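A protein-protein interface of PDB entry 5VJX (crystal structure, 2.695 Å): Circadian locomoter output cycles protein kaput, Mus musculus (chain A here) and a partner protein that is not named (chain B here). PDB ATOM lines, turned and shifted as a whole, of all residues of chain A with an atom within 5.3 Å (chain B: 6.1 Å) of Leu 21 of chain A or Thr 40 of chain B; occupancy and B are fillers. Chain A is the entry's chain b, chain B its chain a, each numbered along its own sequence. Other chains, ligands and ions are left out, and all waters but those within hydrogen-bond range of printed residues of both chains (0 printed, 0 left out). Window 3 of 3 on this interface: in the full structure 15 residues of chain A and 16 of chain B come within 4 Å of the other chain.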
ATOM      1  N   HIS A  16      -2.895 -22.665  23.513  1.00  0.00           N
ATOM      2  CA  HIS A  16      -4.062 -23.540  23.546  1.00  0.00           C
ATOM      3  C   HIS A  16      -4.367 -24.050  22.130  1.00  0.00           C
ATOM      4  O   HIS A  16      -4.564 -25.258  21.915  1.00  0.00           O
ATOM      5  CB  HIS A  16      -5.254 -22.799  24.166  1.00  0.00           C
ATOM      6  CG  HIS A  16      -6.461 -23.655  24.404  1.00  0.00           C
ATOM      7  ND1 HIS A  16      -7.500 -23.761  23.506  1.00  0.00           N
ATOM      8  CD2 HIS A  16      -6.795 -24.440  25.456  1.00  0.00           C
ATOM      9  CE1 HIS A  16      -8.420 -24.574  23.992  1.00  0.00           C
ATOM     10  NE2 HIS A  16      -8.016 -25.002  25.174  1.00  0.00           N
ATOM     11  N   LEU A  17      -4.326 -23.141  21.158  1.00  0.00           N
ATOM     12  CA  LEU A  17      -4.635 -23.491  19.770  1.00  0.00           C
ATOM     13  C   LEU A  17      -3.618 -24.459  19.196  1.00  0.00           C
ATOM     14  O   LEU A  17      -3.972 -25.427  18.517  1.00  0.00           O
ATOM     15  CB  LEU A  17      -4.663 -22.244  18.892  1.00  0.00           C
ATOM     16  CG  LEU A  17      -5.760 -21.203  19.074  1.00  0.00           C
ATOM     17  CD1 LEU A  17      -5.414 -19.947  18.296  1.00  0.00           C
ATOM     18  CD2 LEU A  17      -7.072 -21.763  18.594  1.00  0.00           C
ATOM     19  N   LYS A  18      -2.352 -24.195  19.486  1.00  0.00           N
ATOM     20  CA  LYS A  18      -1.269 -25.043  19.031  1.00  0.00           C
ATOM     21  C   LYS A  18      -1.416 -26.427  19.628  1.00  0.00           C
ATOM     22  O   LYS A  18      -1.111 -27.433  18.982  1.00  0.00           O
ATOM     23  CB  LYS A  18       0.076 -24.439  19.424  1.00  0.00           C
ATOM     24  CG  LYS A  18       1.281 -25.255  19.008  1.00  0.00           C
ATOM     25  CD  LYS A  18       2.558 -24.605  19.503  1.00  0.00           C
ATOM     26  CE  LYS A  18       3.793 -25.354  19.033  1.00  0.00           C
ATOM     27  NZ  LYS A  18       3.934 -26.675  19.707  1.00  0.00           N
ATOM     28  N   ASP A  19      -1.944 -26.482  20.845  1.00  0.00           N
ATOM     29  CA  ASP A  19      -2.079 -27.756  21.525  1.00  0.00           C
ATOM     30  C   ASP A  19      -3.183 -28.589  20.916  1.00  0.00           C
ATOM     31  O   ASP A  19      -3.001 -29.785  20.677  1.00  0.00           O
ATOM     32  CB  ASP A  19      -2.348 -27.553  23.014  1.00  0.00           C
ATOM     33  CG  ASP A  19      -1.117 -27.113  23.770  1.00  0.00           C
ATOM     34  OD1 ASP A  19      -0.016 -27.161  23.188  1.00  0.00           O
ATOM     35  OD2 ASP A  19      -1.243 -26.735  24.952  1.00  0.00           O
ATOM     36  N   GLN A  20      -4.330 -27.976  20.659  1.00  0.00           N
ATOM     37  CA  GLN A  20      -5.404 -28.749  20.051  1.00  0.00           C
ATOM     38  C   GLN A  20      -5.021 -29.184  18.635  1.00  0.00           C
ATOM     39  O   GLN A  20      -5.370 -30.284  18.188  1.00  0.00           O
ATOM     40  CB  GLN A  20      -6.703 -27.978  20.028  1.00  0.00           C
ATOM     41  CG  GLN A  20      -7.853 -28.859  19.631  1.00  0.00           C
ATOM     42  CD  GLN A  20      -9.151 -28.117  19.638  1.00  0.00           C
ATOM     43  OE1 GLN A  20      -9.450 -27.402  20.595  1.00  0.00           O
ATOM     44  NE2 GLN A  20      -9.988 -28.373  18.638  1.00  0.00           N
ATOM     45  N   LEU A  21      -4.309 -28.312  17.926  1.00  0.00           N
ATOM     46  CA  LEU A  21      -3.915 -28.612  16.554  1.00  0.00           C
ATOM     47  C   LEU A  21      -2.963 -29.818  16.552  1.00  0.00           C
ATOM     48  O   LEU A  21      -3.136 -30.780  15.785  1.00  0.00           O
ATOM     49  CB  LEU A  21      -3.240 -27.383  15.929  1.00  0.00           C
ATOM     50  CG  LEU A  21      -2.978 -27.234  14.432  1.00  0.00           C
ATOM     51  CD1 LEU A  21      -4.283 -27.116  13.686  1.00  0.00           C
ATOM     52  CD2 LEU A  21      -2.109 -26.022  14.185  1.00  0.00           C
ATOM     53  N   GLU A  22      -2.001 -29.801  17.472  1.00  0.00           N
ATOM     54  CA  GLU A  22      -1.067 -30.920  17.601  1.00  0.00           C
ATOM     55  C   GLU A  22      -1.785 -32.194  18.029  1.00  0.00           C
ATOM     56  O   GLU A  22      -1.407 -33.301  17.633  1.00  0.00           O
ATOM     57  CB  GLU A  22       0.048 -30.593  18.590  1.00  0.00           C
ATOM     58  CG  GLU A  22       1.051 -29.578  18.072  1.00  0.00           C
ATOM     59  CD  GLU A  22       2.148 -29.275  19.078  1.00  0.00           C
ATOM     60  OE1 GLU A  22       2.066 -29.776  20.219  1.00  0.00           O
ATOM     61  OE2 GLU A  22       3.096 -28.538  18.730  1.00  0.00           O
ATOM     62  N   GLN A  23      -2.825 -32.037  18.837  1.00  0.00           N
ATOM     63  CA  GLN A  23      -3.563 -33.191  19.311  1.00  0.00           C
ATOM     64  C   GLN A  23      -4.257 -33.832  18.128  1.00  0.00           C
ATOM     65  O   GLN A  23      -4.366 -35.065  18.039  1.00  0.00           O
ATOM     66  CB  GLN A  23      -4.563 -32.805  20.395  1.00  0.00           C
ATOM     67  CG  GLN A  23      -5.231 -34.004  21.027  1.00  0.00           C
ATOM     68  CD  GLN A  23      -4.227 -35.027  21.497  1.00  0.00           C
ATOM     69  OE1 GLN A  23      -3.262 -34.701  22.186  1.00  0.00           O
ATOM     70  NE2 GLN A  23      -4.431 -36.273  21.094  1.00  0.00           N
ATOM     71  N   ARG A  24      -4.672 -32.990  17.188  1.00  0.00           N
ATOM     72  CA  ARG A  24      -5.326 -33.490  15.992  1.00  0.00           C
ATOM     73  C   ARG A  24      -4.296 -34.241  15.175  1.00  0.00           C
ATOM     74  O   ARG A  24      -4.594 -35.282  14.568  1.00  0.00           O
ATOM     75  CB  ARG A  24      -5.908 -32.362  15.159  1.00  0.00           C
ATOM     76  CG  ARG A  24      -7.111 -31.691  15.751  1.00  0.00           C
ATOM     77  CD  ARG A  24      -7.561 -30.633  14.788  1.00  0.00           C
ATOM     78  NE  ARG A  24      -7.911 -31.266  13.521  1.00  0.00           N
ATOM     79  CZ  ARG A  24      -8.209 -30.609  12.408  1.00  0.00           C
ATOM     80  NH1 ARG A  24      -8.176 -29.284  12.388  1.00  0.00           N
ATOM     81  NH2 ARG A  24      -8.517 -31.280  11.308  1.00  0.00           N
ATOM     82  N   THR A  25      -3.070 -33.725  15.189  1.00  0.00           N
ATOM     83  CA  THR A  25      -1.982 -34.404  14.502  1.00  0.00           C
ATOM     84  C   THR A  25      -1.738 -35.811  15.033  1.00  0.00           C
ATOM     85  O   THR A  25      -1.617 -36.762  14.258  1.00  0.00           O
ATOM     86  CB  THR A  25      -0.672 -33.616  14.634  1.00  0.00           C
ATOM     87  OG1 THR A  25      -0.604 -32.627  13.606  1.00  0.00           O
ATOM     88  CG2 THR A  25       0.513 -34.528  14.491  1.00  0.00           C
ATOM     89  N   GLN B  35      -7.428 -30.967   5.602  1.00  0.00           N
ATOM     90  CA  GLN B  35      -7.969 -29.872   6.417  1.00  0.00           C
ATOM     91  C   GLN B  35      -7.015 -29.420   7.524  1.00  0.00           C
ATOM     92  O   GLN B  35      -6.826 -28.217   7.765  1.00  0.00           O
ATOM     93  CB  GLN B  35      -9.307 -30.252   7.041  1.00  0.00           C
ATOM     94  CG  GLN B  35      -9.995 -29.059   7.674  1.00  0.00           C
ATOM     95  CD  GLN B  35     -11.403 -29.357   8.114  1.00  0.00           C
ATOM     96  OE1 GLN B  35     -11.901 -30.467   7.930  1.00  0.00           O
ATOM     97  NE2 GLN B  35     -12.050 -28.374   8.726  1.00  0.00           N
ATOM     98  N   LEU B  36      -6.425 -30.388   8.214  1.00  0.00           N
ATOM     99  CA  LEU B  36      -5.480 -30.064   9.266  1.00  0.00           C
ATOM    100  C   LEU B  36      -4.311 -29.307   8.643  1.00  0.00           C
ATOM    101  O   LEU B  36      -3.748 -28.403   9.255  1.00  0.00           O
ATOM    102  CB  LEU B  36      -4.996 -31.326   9.972  1.00  0.00           C
ATOM    103  CG  LEU B  36      -3.960 -31.141  11.077  1.00  0.00           C
ATOM    104  CD1 LEU B  36      -4.587 -30.402  12.231  1.00  0.00           C
ATOM    105  CD2 LEU B  36      -3.444 -32.484  11.520  1.00  0.00           C
ATOM    106  N   LYS B  37      -3.969 -29.674   7.409  1.00  0.00           N
ATOM    107  CA  LYS B  37      -2.902 -28.999   6.682  1.00  0.00           C
ATOM    108  C   LYS B  37      -3.240 -27.553   6.384  1.00  0.00           C
ATOM    109  O   LYS B  37      -2.401 -26.680   6.540  1.00  0.00           O
ATOM    110  CB  LYS B  37      -2.600 -29.701   5.360  1.00  0.00           C
ATOM    111  CG  LYS B  37      -1.549 -28.971   4.535  1.00  0.00           C
ATOM    112  CD  LYS B  37      -1.287 -29.621   3.188  1.00  0.00           C
ATOM    113  CE  LYS B  37      -0.394 -28.724   2.346  1.00  0.00           C
ATOM    114  NZ  LYS B  37      -0.818 -27.302   2.475  1.00  0.00           N
ATOM    115  N   GLU B  38      -4.471 -27.298   5.960  1.00  0.00           N
ATOM    116  CA  GLU B  38      -4.860 -25.938   5.627  1.00  0.00           C
ATOM    117  C   GLU B  38      -4.913 -25.065   6.869  1.00  0.00           C
ATOM    118  O   GLU B  38      -4.563 -23.891   6.797  1.00  0.00           O
ATOM    119  CB  GLU B  38      -6.191 -25.917   4.859  1.00  0.00           C
ATOM    120  CG  GLU B  38      -7.449 -26.231   5.622  1.00  0.00           C
ATOM    121  CD  GLU B  38      -8.665 -26.203   4.721  1.00  0.00           C
ATOM    122  OE1 GLU B  38      -8.578 -25.598   3.633  1.00  0.00           O
ATOM    123  OE2 GLU B  38      -9.700 -26.798   5.088  1.00  0.00           O
ATOM    124  N   GLN B  39      -5.390 -25.605   7.990  1.00  0.00           N
ATOM    125  CA  GLN B  39      -5.409 -24.806   9.215  1.00  0.00           C
ATOM    126  C   GLN B  39      -3.984 -24.533   9.723  1.00  0.00           C
ATOM    127  O   GLN B  39      -3.699 -23.446  10.225  1.00  0.00           O
ATOM    128  CB  GLN B  39      -6.266 -25.475  10.275  1.00  0.00           C
ATOM    129  CG  GLN B  39      -7.734 -25.288   9.978  1.00  0.00           C
ATOM    130  CD  GLN B  39      -8.625 -26.199  10.774  1.00  0.00           C
ATOM    131  OE1 GLN B  39      -8.164 -27.130  11.427  1.00  0.00           O
ATOM    132  NE2 GLN B  39      -9.921 -25.930  10.732  1.00  0.00           N
ATOM    133  N   THR B  40      -3.097 -25.523   9.635  1.00  0.00           N
ATOM    134  CA  THR B  40      -1.668 -25.261   9.806  1.00  0.00           C
ATOM    135  C   THR B  40      -1.325 -24.447   8.548  1.00  0.00           C
ATOM    136  O   THR B  40      -2.160 -24.363   7.656  1.00  0.00           O
ATOM    137  CB  THR B  40      -0.839 -26.548   9.940  1.00  0.00           C
ATOM    138  OG1 THR B  40      -1.313 -27.305  11.058  1.00  0.00           O
ATOM    139  CG2 THR B  40       0.627 -26.235  10.160  1.00  0.00           C
ATOM    140  N   GLN B  41      -0.141 -23.843   8.435  1.00  0.00           N
ATOM    141  CA  GLN B  41       0.171 -23.055   7.230  1.00  0.00           C
ATOM    142  C   GLN B  41      -0.845 -21.912   7.124  1.00  0.00           C
ATOM    143  O   GLN B  41      -1.010 -21.305   6.073  1.00  0.00           O
ATOM    144  CB  GLN B  41       0.154 -23.925   5.954  1.00  0.00           C
ATOM    145  CG  GLN B  41       1.244 -25.001   5.832  1.00  0.00           C
ATOM    146  CD  GLN B  41       2.557 -24.474   5.256  1.00  0.00           C
ATOM    147  OE1 GLN B  41       3.466 -24.079   5.989  1.00  0.00           O
ATOM    148  NE2 GLN B  41       2.665 -24.491   3.927  1.00  0.00           N
ATOM    149  N   MET B  42      -1.535 -21.667   8.236  1.00  0.00           N
ATOM    150  CA  MET B  42      -2.496 -20.588   8.413  1.00  0.00           C
ATOM    151  C   MET B  42      -2.431 -20.213   9.878  1.00  0.00           C
ATOM    152  O   MET B  42      -2.638 -19.063  10.257  1.00  0.00           O
ATOM    153  CB  MET B  42      -3.916 -21.005   8.026  1.00  0.00           C
ATOM    154  CG  MET B  42      -4.994 -20.032   8.508  1.00  0.00           C
ATOM    155  SD  MET B  42      -6.787 -20.389   7.823  1.00  0.00           S
ATOM    156  CE  MET B  42      -6.295 -20.904   6.007  1.00  0.00           C
ATOM    157  N   PHE B  43      -2.135 -21.208  10.706  1.00  0.00           N
ATOM    158  CA  PHE B  43      -1.856 -20.952  12.104  1.00  0.00           C
ATOM    159  C   PHE B  43      -0.524 -20.257  12.234  1.00  0.00           C
ATOM    160  O   PHE B  43      -0.433 -19.135  12.723  1.00  0.00           O
ATOM    161  CB  PHE B  43      -1.807 -22.255  12.899  1.00  0.00           C
ATOM    162  CG  PHE B  43      -1.426 -22.064  14.338  1.00  0.00           C
ATOM    163  CD1 PHE B  43      -2.096 -21.150  15.123  1.00  0.00           C
ATOM    164  CD2 PHE B  43      -0.365 -22.761  14.889  1.00  0.00           C
ATOM    165  CE1 PHE B  43      -1.750 -20.969  16.431  1.00  0.00           C
ATOM    166  CE2 PHE B  43      -0.007 -22.572  16.207  1.00  0.00           C
ATOM    167  CZ  PHE B  43      -0.703 -21.671  16.976  1.00  0.00           C
ATOM    168  N   ILE B  44       0.505 -20.949  11.757  1.00  0.00           N
ATOM    169  CA  ILE B  44       1.868 -20.452  11.744  1.00  0.00           C
ATOM    170  C   ILE B  44       1.949 -19.154  10.929  1.00  0.00           C
ATOM    171  O   ILE B  44       2.880 -18.381  11.091  1.00  0.00           O
ATOM    172  CB  ILE B  44       2.830 -21.529  11.183  1.00  0.00           C
ATOM    173  CG1 ILE B  44       2.618 -22.859  11.906  1.00  0.00           C
ATOM    174  CG2 ILE B  44       4.283 -21.076  11.245  1.00  0.00           C
ATOM    175  CD1 ILE B  44       2.884 -22.805  13.381  1.00  0.00           C
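OG1 of Thr 40 of chain B lies within hydrogen-bond range of O of Leu 36 of chain B, at 3.2 Å. OE1 of Glu 22 of chain A lies within salt-bridge range of NZ of Lys 18 of chain A (3.7 Å).
Of the printed residues of chain B, Lys 18 of chain A touches Phe 43. Leu 21 of chain A touches just these residues of chain B: Leu 36 (3.6 Å), Thr 40 (3.5 Å) and Phe 43 (3.8 Å). Printed residues of chain B within 4 Å of Arg 24 of chain A: Leu 36 and Gln 39. Of the printed residues of chain B, Thr 25 of chain A touches Leu 36 (3.5 Å). Printed residues of chain A within 4 Å of Leu 36 of chain B: Leu 21, Arg 24 and Thr 25. The nearest residue of chain B that does not touch Leu 21 of chain A is Gln 39 of chain B (4.3 Å). The nearest printed residue of chain A that does not touch Thr 40 of chain B is Thr 25 of chain A (5.9 Å). The nearest printed residue of chain A that does not touch Gln 39 of chain B is Leu 21 of chain A (4.3 Å).
Hydrophobic or aromatic side chains of chain B within 4 Å of the printed part of chain A: Leu 36 and Phe 43. Hydrophobic or aromatic side chains of chain A within 4 Å of the printed part of chain B: Leu 21. Among the printed residues, 7 pairs touch across the chains. Among the printed residues, no Asp or Glu carboxylate lies within 4 Å of a Lys or Arg side-chain nitrogen of the other chain.
Among the printed residues, merely in contact across the chains: Leu 21 of chain A with Thr 40 of chain B (3.5 Å), Thr 25 of chain A with Leu 36 of chain B (3.5 Å), Leu 21 of chain A with Leu 36 of chain B (3.6 Å), Arg 24 of chain A with Leu 36 of chain B (3.6 Å), Lys 18 of chain A with Phe 43 of chain B (3.7 Å) and Leu 21 of chain A with Phe 43 of chain B (3.8 Å).
The guanidinium group (NH1) of Arg 24 of chain A sits close to the side-chain amide oxygen (OE1) of Gln 39 of chain B, 2.4 Å away.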
